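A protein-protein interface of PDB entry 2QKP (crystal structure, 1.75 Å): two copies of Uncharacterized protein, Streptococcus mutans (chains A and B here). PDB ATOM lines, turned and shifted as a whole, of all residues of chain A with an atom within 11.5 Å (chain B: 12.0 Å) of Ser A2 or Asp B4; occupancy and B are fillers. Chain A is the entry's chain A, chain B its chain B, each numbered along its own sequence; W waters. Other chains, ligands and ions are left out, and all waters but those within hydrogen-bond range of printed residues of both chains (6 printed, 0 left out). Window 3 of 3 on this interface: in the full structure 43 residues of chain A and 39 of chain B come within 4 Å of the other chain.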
ATOM      1  N   SER A   2      -8.553  12.777 -22.042  1.00  0.00           N
ATOM      2  CA  SER A   2      -8.314  13.075 -23.475  1.00  0.00           C
ATOM      3  C   SER A   2      -9.124  14.282 -23.887  1.00  0.00           C
ATOM      4  O   SER A   2     -10.013  14.726 -23.146  1.00  0.00           O
ATOM      5  CB  SER A   2      -8.686  11.888 -24.345  1.00  0.00           C
ATOM      6  OG  SER A   2      -9.994  11.454 -24.052  1.00  0.00           O
ATOM      7  N   LEU A   3      -8.799  14.816 -25.065  1.00  0.00           N
ATOM      8  CA  LEU A   3      -9.492  15.976 -25.601  1.00  0.00           C
ATOM      9  C   LEU A   3      -9.339  15.981 -27.106  1.00  0.00           C
ATOM     10  O   LEU A   3      -8.233  15.862 -27.638  1.00  0.00           O
ATOM     11  CB  LEU A   3      -8.937  17.273 -24.999  1.00  0.00           C
ATOM     12  CG  LEU A   3      -9.824  18.510 -25.163  1.00  0.00           C
ATOM     13  CD1 LEU A   3     -11.067  18.428 -24.300  1.00  0.00           C
ATOM     14  CD2 LEU A   3      -9.040  19.781 -24.810  1.00  0.00           C
ATOM     15  N   ASP A   4     -10.466  16.093 -27.806  1.00  0.00           N
ATOM     16  CA  ASP A   4     -10.406  16.114 -29.263  1.00  0.00           C
ATOM     17  C   ASP A   4      -9.840  17.445 -29.778  1.00  0.00           C
ATOM     18  O   ASP A   4      -9.586  18.373 -29.005  1.00  0.00           O
ATOM     19  CB  ASP A   4     -11.769  15.757 -29.904  1.00  0.00           C
ATOM     20  CG  ASP A   4     -12.853  16.754 -29.577  1.00  0.00           C
ATOM     21  OD1 ASP A   4     -12.518  17.938 -29.341  1.00  0.00           O
ATOM     22  OD2 ASP A   4     -14.053  16.376 -29.571  1.00  0.00           O
ATOM     23  N   ARG A   5      -9.630  17.502 -31.083  1.00  0.00           N
ATOM     24  CA  ARG A   5      -8.875  18.599 -31.687  1.00  0.00           C
ATOM     25  C   ARG A   5      -9.672  19.865 -31.824  1.00  0.00           C
ATOM     26  O   ARG A   5      -9.094  20.925 -32.093  1.00  0.00           O
ATOM     27  CB  ARG A   5      -8.376  18.176 -33.063  1.00  0.00           C
ATOM     28  CG  ARG A   5      -7.273  17.158 -32.985  1.00  0.00           C
ATOM     29  CD  ARG A   5      -6.759  16.837 -34.399  1.00  0.00           C
ATOM     30  NE  ARG A   5      -6.240  18.000 -35.132  1.00  0.00           N
ATOM     31  CZ  ARG A   5      -4.946  18.363 -35.173  1.00  0.00           C
ATOM     32  NH1 ARG A   5      -4.028  17.678 -34.507  1.00  0.00           N
ATOM     33  NH2 ARG A   5      -4.575  19.420 -35.906  1.00  0.00           N
ATOM     34  N   THR A   6     -11.002  19.779 -31.683  1.00  0.00           N
ATOM     35  CA  THR A   6     -11.833  20.952 -31.970  1.00  0.00           C
ATOM     36  C   THR A   6     -12.459  21.576 -30.728  1.00  0.00           C
ATOM     37  O   THR A   6     -13.140  22.641 -30.831  1.00  0.00           O
ATOM     38  CB  THR A   6     -12.929  20.625 -33.037  1.00  0.00           C
ATOM     39  OG1 THR A   6     -13.835  19.679 -32.461  1.00  0.00           O
ATOM     40  CG2 THR A   6     -12.254  20.074 -34.289  1.00  0.00           C
ATOM     41  N   THR A   7     -12.229  20.960 -29.561  1.00  0.00           N
ATOM     42  CA  THR A   7     -12.749  21.491 -28.288  1.00  0.00           C
ATOM     43  C   THR A   7     -11.802  22.514 -27.672  1.00  0.00           C
ATOM     44  O   THR A   7     -10.569  22.304 -27.644  1.00  0.00           O
ATOM     45  CB  THR A   7     -13.065  20.350 -27.273  1.00  0.00           C
ATOM     46  OG1 THR A   7     -14.000  19.429 -27.872  1.00  0.00           O
ATOM     47  CG2 THR A   7     -13.645  20.887 -25.936  1.00  0.00           C
ATOM     48  N   GLN A   8     -12.378  23.608 -27.173  1.00  0.00           N
ATOM     49  CA  GLN A   8     -11.570  24.703 -26.560  1.00  0.00           C
ATOM     50  C   GLN A   8     -10.809  24.244 -25.348  1.00  0.00           C
ATOM     51  O   GLN A   8     -11.292  23.398 -24.577  1.00  0.00           O
ATOM     52  CB  GLN A   8     -12.465  25.878 -26.158  1.00  0.00           C
ATOM     53  CG  GLN A   8     -13.181  26.511 -27.322  1.00  0.00           C
ATOM     54  CD  GLN A   8     -12.246  26.895 -28.404  1.00  0.00           C
ATOM     55  OE1 GLN A   8     -11.241  27.559 -28.152  1.00  0.00           O
ATOM     56  NE2 GLN A   8     -12.547  26.484 -29.632  1.00  0.00           N
ATOM     57  N   GLN A   9      -9.581  24.753 -25.212  1.00  0.00           N
ATOM     58  CA  GLN A   9      -8.787  24.511 -24.009  1.00  0.00           C
ATOM     59  C   GLN A   9      -7.887  25.715 -23.756  1.00  0.00           C
ATOM     60  O   GLN A   9      -7.700  26.527 -24.642  1.00  0.00           O
ATOM     61  CB  GLN A   9      -7.933  23.260 -24.147  1.00  0.00           C
ATOM     62  CG  GLN A   9      -6.950  23.238 -25.321  1.00  0.00           C
ATOM     63  CD  GLN A   9      -6.244  21.915 -25.393  1.00  0.00           C
ATOM     64  OE1 GLN A   9      -5.470  21.571 -24.492  1.00  0.00           O
ATOM     65  NE2 GLN A   9      -6.505  21.152 -26.446  1.00  0.00           N
ATOM     66  N   PRO A  10      -7.360  25.846 -22.529  1.00  0.00           N
ATOM     67  CA  PRO A  10      -6.562  27.042 -22.301  1.00  0.00           C
ATOM     68  C   PRO A  10      -5.340  27.148 -23.217  1.00  0.00           C
ATOM     69  O   PRO A  10      -4.616  26.162 -23.440  1.00  0.00           O
ATOM     70  CB  PRO A  10      -6.126  26.913 -20.840  1.00  0.00           C
ATOM     71  CG  PRO A  10      -7.163  26.044 -20.229  1.00  0.00           C
ATOM     72  CD  PRO A  10      -7.560  25.062 -21.301  1.00  0.00           C
ATOM     73  N   PHE A  11      -5.133  28.342 -23.746  1.00  0.00           N
ATOM     74  CA  PHE A  11      -3.893  28.671 -24.470  1.00  0.00           C
ATOM     75  C   PHE A  11      -3.605  30.108 -24.094  1.00  0.00           C
ATOM     76  O   PHE A  11      -4.515  30.949 -24.117  1.00  0.00           O
ATOM     77  CB  PHE A  11      -4.123  28.606 -25.977  1.00  0.00           C
ATOM     78  CG  PHE A  11      -3.744  27.282 -26.636  1.00  0.00           C
ATOM     79  CD1 PHE A  11      -2.471  27.112 -27.220  1.00  0.00           C
ATOM     80  CD2 PHE A  11      -4.673  26.235 -26.716  1.00  0.00           C
ATOM     81  CE1 PHE A  11      -2.130  25.890 -27.885  1.00  0.00           C
ATOM     82  CE2 PHE A  11      -4.361  25.047 -27.351  1.00  0.00           C
ATOM     83  CZ  PHE A  11      -3.093  24.874 -27.973  1.00  0.00           C
ATOM     84  N   LEU A  16      -8.127  28.254 -27.006  1.00  0.00           N
ATOM     85  CA  LEU A  16      -8.132  27.853 -28.422  1.00  0.00           C
ATOM     86  C   LEU A  16      -8.358  26.355 -28.444  1.00  0.00           C
ATOM     87  O   LEU A  16      -8.001  25.666 -27.490  1.00  0.00           O
ATOM     88  CB  LEU A  16      -6.776  28.095 -29.091  1.00  0.00           C
ATOM     89  CG  LEU A  16      -6.314  29.553 -29.220  1.00  0.00           C
ATOM     90  CD1 LEU A  16      -4.868  29.577 -29.682  1.00  0.00           C
ATOM     91  CD2 LEU A  16      -7.180  30.328 -30.198  1.00  0.00           C
ATOM     92  N   SER A  17      -8.883  25.852 -29.556  1.00  0.00           N
ATOM     93  CA  SER A  17      -8.796  24.404 -29.809  1.00  0.00           C
ATOM     94  C   SER A  17      -7.452  24.170 -30.503  1.00  0.00           C
ATOM     95  O   SER A  17      -6.851  25.100 -30.989  1.00  0.00           O
ATOM     96  CB  SER A  17      -9.945  23.978 -30.734  1.00  0.00           C
ATOM     97  OG  SER A  17      -9.816  24.603 -31.995  1.00  0.00           O
ATOM     98  N   VAL A  18      -6.990  22.924 -30.555  1.00  0.00           N
ATOM     99  CA  VAL A  18      -5.841  22.544 -31.346  1.00  0.00           C
ATOM    100  C   VAL A  18      -6.032  22.955 -32.821  1.00  0.00           C
ATOM    101  O   VAL A  18      -5.115  23.524 -33.429  1.00  0.00           O
ATOM    102  CB  VAL A  18      -5.593  20.995 -31.262  1.00  0.00           C
ATOM    103  CG1 VAL A  18      -4.671  20.535 -32.408  1.00  0.00           C
ATOM    104  CG2 VAL A  18      -4.990  20.630 -29.920  1.00  0.00           C
ATOM    105  N   LEU B   3      -0.837  12.189 -20.530  1.00  0.00           N
ATOM    106  CA  LEU B   3      -1.364  13.574 -20.378  1.00  0.00           C
ATOM    107  C   LEU B   3      -1.630  14.240 -21.734  1.00  0.00           C
ATOM    108  O   LEU B   3      -0.822  14.188 -22.684  1.00  0.00           O
ATOM    109  CB  LEU B   3      -0.487  14.437 -19.453  1.00  0.00           C
ATOM    110  CG  LEU B   3      -0.837  15.923 -19.297  1.00  0.00           C
ATOM    111  CD1 LEU B   3      -1.873  16.194 -18.211  1.00  0.00           C
ATOM    112  CD2 LEU B   3       0.410  16.720 -19.023  1.00  0.00           C
ATOM    113  N   ASP B   4      -2.809  14.843 -21.794  1.00  0.00           N
ATOM    114  CA  ASP B   4      -3.346  15.403 -23.005  1.00  0.00           C
ATOM    115  C   ASP B   4      -2.537  16.600 -23.493  1.00  0.00           C
ATOM    116  O   ASP B   4      -2.509  16.829 -24.688  1.00  0.00           O
ATOM    117  CB  ASP B   4      -4.788  15.846 -22.779  1.00  0.00           C
ATOM    118  CG  ASP B   4      -5.733  14.679 -22.515  1.00  0.00           C
ATOM    119  OD1 ASP B   4      -5.415  13.523 -22.916  1.00  0.00           O
ATOM    120  OD2 ASP B   4      -6.803  14.938 -21.915  1.00  0.00           O
ATOM    121  N   ARG B   5      -1.923  17.357 -22.582  1.00  0.00           N
ATOM    122  CA  ARG B   5      -1.162  18.566 -22.983  1.00  0.00           C
ATOM    123  C   ARG B   5       0.254  18.238 -23.433  1.00  0.00           C
ATOM    124  O   ARG B   5       0.902  19.075 -24.056  1.00  0.00           O
ATOM    125  CB  ARG B   5      -1.096  19.631 -21.876  1.00  0.00           C
ATOM    126  CG  ARG B   5      -2.313  20.551 -21.767  1.00  0.00           C
ATOM    127  CD  ARG B   5      -2.070  21.738 -20.818  1.00  0.00           C
ATOM    128  NE  ARG B   5      -1.541  22.929 -21.504  1.00  0.00           N
ATOM    129  CZ  ARG B   5      -0.273  23.349 -21.448  1.00  0.00           C
ATOM    130  NH1 ARG B   5       0.093  24.441 -22.105  1.00  0.00           N
ATOM    131  NH2 ARG B   5       0.635  22.697 -20.732  1.00  0.00           N
ATOM    132  N   THR B   6       0.742  17.032 -23.112  1.00  0.00           N
ATOM    133  CA  THR B   6       2.123  16.660 -23.499  1.00  0.00           C
ATOM    134  C   THR B   6       2.172  15.685 -24.670  1.00  0.00           C
ATOM    135  O   THR B   6       3.233  15.467 -25.273  1.00  0.00           O
ATOM    136  CB  THR B   6       2.899  16.102 -22.303  1.00  0.00           C
ATOM    137  OG1 THR B   6       2.239  14.920 -21.829  1.00  0.00           O
ATOM    138  CG2 THR B   6       2.925  17.126 -21.186  1.00  0.00           C
ATOM    139  N   THR B   7       1.021  15.126 -25.022  1.00  0.00           N
ATOM    140  CA  THR B   7       0.920  14.180 -26.138  1.00  0.00           C
ATOM    141  C   THR B   7       1.152  14.873 -27.485  1.00  0.00           C
ATOM    142  O   THR B   7       0.604  15.944 -27.742  1.00  0.00           O
ATOM    143  CB  THR B   7      -0.458  13.489 -26.140  1.00  0.00           C
ATOM    144  OG1 THR B   7      -0.649  12.850 -24.871  1.00  0.00           O
ATOM    145  CG2 THR B   7      -0.550  12.456 -27.249  1.00  0.00           C
ATOM    146  N   GLN B   8       1.984  14.261 -28.323  1.00  0.00           N
ATOM    147  CA  GLN B   8       2.251  14.824 -29.655  1.00  0.00           C
ATOM    148  C   GLN B   8       1.048  14.678 -30.573  1.00  0.00           C
ATOM    149  O   GLN B   8       0.433  13.599 -30.635  1.00  0.00           O
ATOM    150  CB  GLN B   8       3.507  14.196 -30.258  1.00  0.00           C
ATOM    151  CG  GLN B   8       4.742  14.487 -29.460  1.00  0.00           C
ATOM    152  CD  GLN B   8       5.116  15.960 -29.535  1.00  0.00           C
ATOM    153  OE1 GLN B   8       4.929  16.600 -30.585  1.00  0.00           O
ATOM    154  NE2 GLN B   8       5.640  16.502 -28.435  1.00  0.00           N
ATOM    155  N   GLN B   9       0.675  15.771 -31.239  1.00  0.00           N
ATOM    156  CA  GLN B   9      -0.462  15.812 -32.164  1.00  0.00           C
ATOM    157  C   GLN B   9      -0.021  16.440 -33.475  1.00  0.00           C
ATOM    158  O   GLN B   9       0.889  17.283 -33.473  1.00  0.00           O
ATOM    159  CB  GLN B   9      -1.576  16.692 -31.587  1.00  0.00           C
ATOM    160  CG  GLN B   9      -1.996  16.284 -30.208  1.00  0.00           C
ATOM    161  CD  GLN B   9      -3.262  16.962 -29.790  1.00  0.00           C
ATOM    162  OE1 GLN B   9      -4.263  16.995 -30.533  1.00  0.00           O
ATOM    163  NE2 GLN B   9      -3.240  17.521 -28.605  1.00  0.00           N
ATOM    164  N   PRO B  10      -0.664  16.076 -34.595  1.00  0.00           N
ATOM    165  CA  PRO B  10      -0.333  16.753 -35.848  1.00  0.00           C
ATOM    166  C   PRO B  10      -0.575  18.263 -35.782  1.00  0.00           C
ATOM    167  O   PRO B  10      -1.640  18.719 -35.345  1.00  0.00           O
ATOM    168  CB  PRO B  10      -1.292  16.114 -36.875  1.00  0.00           C
ATOM    169  CG  PRO B  10      -1.575  14.748 -36.270  1.00  0.00           C
ATOM    170  CD  PRO B  10      -1.667  15.010 -34.793  1.00  0.00           C
ATOM    171  N   PHE B  11       0.444  19.011 -36.181  1.00  0.00           N
ATOM    172  CA  PHE B  11       0.371  20.466 -36.322  1.00  0.00           C
ATOM    173  C   PHE B  11       1.172  20.767 -37.578  1.00  0.00           C
ATOM    174  O   PHE B  11       2.291  20.298 -37.693  1.00  0.00           O
ATOM    175  CB  PHE B  11       1.080  21.139 -35.143  1.00  0.00           C
ATOM    176  CG  PHE B  11       0.191  21.493 -33.980  1.00  0.00           C
ATOM    177  CD1 PHE B  11      -0.364  22.764 -33.878  1.00  0.00           C
ATOM    178  CD2 PHE B  11      -0.018  20.591 -32.963  1.00  0.00           C
ATOM    179  CE1 PHE B  11      -1.172  23.113 -32.763  1.00  0.00           C
ATOM    180  CE2 PHE B  11      -0.783  20.933 -31.846  1.00  0.00           C
ATOM    181  CZ  PHE B  11      -1.377  22.206 -31.775  1.00  0.00           C
ATOM    182  N   TYR B  15       4.645  17.633 -35.899  1.00  0.00           N
ATOM    183  CA  TYR B  15       3.938  17.381 -34.638  1.00  0.00           C
ATOM    184  C   TYR B  15       4.341  18.353 -33.562  1.00  0.00           C
ATOM    185  O   TYR B  15       5.495  18.795 -33.523  1.00  0.00           O
ATOM    186  CB  TYR B  15       4.241  15.976 -34.101  1.00  0.00           C
ATOM    187  CG  TYR B  15       3.603  14.866 -34.883  1.00  0.00           C
ATOM    188  CD1 TYR B  15       4.176  14.422 -36.087  1.00  0.00           C
ATOM    189  CD2 TYR B  15       2.432  14.237 -34.424  1.00  0.00           C
ATOM    190  CE1 TYR B  15       3.592  13.400 -36.823  1.00  0.00           C
ATOM    191  CE2 TYR B  15       1.845  13.201 -35.151  1.00  0.00           C
ATOM    192  CZ  TYR B  15       2.433  12.792 -36.351  1.00  0.00           C
ATOM    193  OH  TYR B  15       1.853  11.773 -37.095  1.00  0.00           O
ATOM    194  N   LEU B  16       3.384  18.665 -32.683  1.00  0.00           N
ATOM    195  CA  LEU B  16       3.647  19.425 -31.467  1.00  0.00           C
ATOM    196  C   LEU B  16       2.667  18.944 -30.441  1.00  0.00           C
ATOM    197  O   LEU B  16       1.549  18.504 -30.778  1.00  0.00           O
ATOM    198  CB  LEU B  16       3.403  20.932 -31.643  1.00  0.00           C
ATOM    199  CG  LEU B  16       4.233  21.752 -32.632  1.00  0.00           C
ATOM    200  CD1 LEU B  16       3.606  23.131 -32.830  1.00  0.00           C
ATOM    201  CD2 LEU B  16       5.660  21.930 -32.113  1.00  0.00           C
ATOM    202  N   SER B  17       3.050  19.071 -29.181  1.00  0.00           N
ATOM    203  CA  SER B  17       2.070  18.938 -28.108  1.00  0.00           C
ATOM    204  C   SER B  17       1.414  20.276 -27.892  1.00  0.00           C
ATOM    205  O   SER B  17       1.919  21.317 -28.339  1.00  0.00           O
ATOM    206  CB  SER B  17       2.780  18.518 -26.815  1.00  0.00           C
ATOM    207  OG  SER B  17       3.653  19.540 -26.387  1.00  0.00           O
ATOM    208  N   VAL B  18       0.290  20.273 -27.192  1.00  0.00           N
ATOM    209  CA  VAL B  18      -0.357  21.542 -26.804  1.00  0.00           C
ATOM    210  C   VAL B  18       0.626  22.409 -26.015  1.00  0.00           C
ATOM    211  O   VAL B  18       0.752  23.611 -26.261  1.00  0.00           O
ATOM    212  CB  VAL B  18      -1.661  21.281 -26.036  1.00  0.00           C
ATOM    213  CG1 VAL B  18      -2.106  22.542 -25.328  1.00  0.00           C
ATOM    214  CG2 VAL B  18      -2.725  20.775 -26.994  1.00  0.00           C
ATOM    215  N   GLU B  19       1.396  21.759 -25.138  1.00  0.00           N
ATOM    216  CA  GLU B  19       2.382  22.480 -24.325  1.00  0.00           C
ATOM    217  C   GLU B  19       3.391  23.240 -25.207  1.00  0.00           C
ATOM    218  O   GLU B  19       3.681  24.431 -24.961  1.00  0.00           O
ATOM    219  CB  GLU B  19       3.094  21.464 -23.423  1.00  0.00           C
ATOM    220  CG  GLU B  19       4.047  22.065 -22.460  1.00  0.00           C
ATOM    221  CD  GLU B  19       4.745  20.976 -21.660  1.00  0.00           C
ATOM    222  OE1 GLU B  19       5.665  20.328 -22.209  1.00  0.00           O
ATOM    223  OE2 GLU B  19       4.326  20.749 -20.508  1.00  0.00           O
ATOM    224  N   GLN B  20       3.916  22.564 -26.235  1.00  0.00           N
ATOM    225  CA  GLN B  20       4.886  23.173 -27.143  1.00  0.00           C
ATOM    226  C   GLN B  20       4.252  24.233 -28.037  1.00  0.00           C
ATOM    227  O   GLN B  20       4.848  25.310 -28.246  1.00  0.00           O
ATOM    228  CB  GLN B  20       5.578  22.122 -27.987  1.00  0.00           C
ATOM    229  CG  GLN B  20       6.419  21.146 -27.148  1.00  0.00           C
ATOM    230  CD  GLN B  20       6.844  19.956 -27.936  1.00  0.00           C
ATOM    231  OE1 GLN B  20       6.090  19.449 -28.765  1.00  0.00           O
ATOM    232  NE2 GLN B  20       8.074  19.488 -27.689  1.00  0.00           N
ATOM    233  N   ALA B  21       3.067  23.943 -28.569  1.00  0.00           N
ATOM    234  CA  ALA B  21       2.374  24.931 -29.427  1.00  0.00           C
ATOM    235  C   ALA B  21       2.150  26.218 -28.630  1.00  0.00           C
ATOM    236  O   ALA B  21       2.357  27.322 -29.138  1.00  0.00           O
ATOM    237  CB  ALA B  21       1.046  24.355 -29.933  1.00  0.00           C
ATOM    238  N   ASN B  22       1.739  26.094 -27.370  1.00  0.00           N
ATOM    239  CA  ASN B  22       1.515  27.260 -26.536  1.00  0.00           C
ATOM    240  C   ASN B  22       2.816  28.043 -26.303  1.00  0.00           C
ATOM    241  O   ASN B  22       2.833  29.291 -26.347  1.00  0.00           O
ATOM    242  CB  ASN B  22       0.904  26.824 -25.198  1.00  0.00           C
ATOM    243  CG  ASN B  22       0.518  27.987 -24.313  1.00  0.00           C
ATOM    244  OD1 ASN B  22      -0.255  28.868 -24.714  1.00  0.00           O
ATOM    245  ND2 ASN B  22       1.062  28.007 -23.090  1.00  0.00           N
HETATM  246  O   HOH W   1      -5.784  13.853 -25.877  1.00  0.00           O
HETATM  247  O   HOH W   2      -4.414  15.225 -32.512  1.00  0.00           O
HETATM  248  O   HOH W   3      -4.280  23.402 -22.482  1.00  0.00           O
HETATM  249  O   HOH W   4      -1.880  25.812 -23.024  1.00  0.00           O
HETATM  250  O   HOH W   5      -4.894  19.063 -23.608  1.00  0.00           O
HETATM  251  O   HOH W   6      -5.523  18.430 -26.803  1.00  0.00           O
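The backbone NH of Ser A2 sits at hydrogen-bond distance from the side-chain carboxylate of Asp B4 (2.8 Å).
The guanidinium group (NH1) of Arg A5 sits at hydrogen-bond distance from the backbone carbonyl oxygen (O) of Pro B10 (2.7 Å).
The backbone NH (N) of Val A18 lies within hydrogen-bond range of the backbone carbonyl oxygen (O) of Arg A5, at 3.3 Å.
N of Gln A9 lies within hydrogen-bond range of O of Leu A16.
The backbone carbonyl oxygen of Arg B5 is in hydrogen-bond range of the backbone NH of Val B18.
The backbone carbonyl oxygen (O) of Leu B16 lies within hydrogen-bond range of the backbone NH (N) of Gln B9.
OD2 of Asp B4 touches N of Leu A3 (3.7 Å).
Arg A5 touches Gln B9 (CG to OE1, 3.9 Å).
Val B18 touches Gln A9 (CG1 to OE1, 3.6 Å).
CG1 of Val B18 touches CZ of Phe A11, at 3.7 Å.
Asn B22 touches Phe A11.
CG2 of Val A18 touches OE1 of Gln B9 (3.8 Å).
Val A18 touches Phe B11.
Val A18 touches Val B18.
Ser A2 touches just one residue of chain B: Asp B4.
Asp B4 touches just these residues of chain A: Ser A2 and Leu A3.
Leu A3 touches one residue of chain B.
No residue of chain B comes within 4 Å of Asp A4.
Of the printed residues of chain A, Gln B9 touches Arg A5 (3.9 Å) and Val A18 (3.8 Å).
Of the printed residues of chain B, Phe A11 touches Val B18 (3.7 Å) and Asn B22 (3.6 Å).
Printed residues of chain B within 4 Å of Arg A5: Gln B9 and Pro B10.
Of the printed residues of chain B, Gln A9 touches Val B18 (3.6 Å).
Arg B5 touches none of the printed residues of chain A.
Ala B21 touches none of the printed residues of chain A.
Of the 13 printed residues of chain A, 6 touch a printed residue of chain B.
Printed residues of chain A that touch a printed residue of chain B: Ser A2, Leu A3, Arg A5, Gln A9, Phe A11 and Val A18.
Printed residues of chain B that touch a printed residue of chain A: Asp B4, Gln B9, Pro B10, Phe B11, Val B18 and Asn B22.
Among the printed residues, no Asp or Glu carboxylate lies within 4 Å of a Lys or Arg side-chain nitrogen of the other chain.
Leu A3 touches Asp B4, but with the chains exchanged Asp A4 does not touch Leu B3 (10.9 Å).
Arg A5 touches Pro B10, but with the chains exchanged Pro A10 does not touch Arg B5 (4.9 Å).
Phe A11 touches Val B18, and with the chains exchanged Val A18 touches Phe B11.
Val B18 touches its own counterpart, Val A18.
12 positions are printed for both chains.
Water W4 bridges the guanidinium group of Arg B5 (2.6 Å) and the backbone carbonyl oxygen of Pro A10 (2.8 Å).
Water W2 bridges the side-chain amide oxygen of Gln B9 (2.7 Å) and the guanidinium group of Arg A5 (3.2 Å).
Water W5 lies within hydrogen-bond range of OE1 of Gln A9 (2.7 Å) and O of Asp B4 (3.4 Å).
Water W6 bridges NE2 of Gln A9 (2.9 Å) and NE2 of Gln B9 (3.0 Å).
Water W3 lies within hydrogen-bond range of the backbone carbonyl oxygen (O) of Pro A10 (2.9 Å), the guanidinium group (NE) of Arg B5 (2.9 Å) and the side-chain amide oxygen (OE1) of Gln A9 (3.0 Å).
Water W1 lies within hydrogen-bond range of OD1 of Asp B4 (3.0 Å) and N of Leu A3 (3.3 Å).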
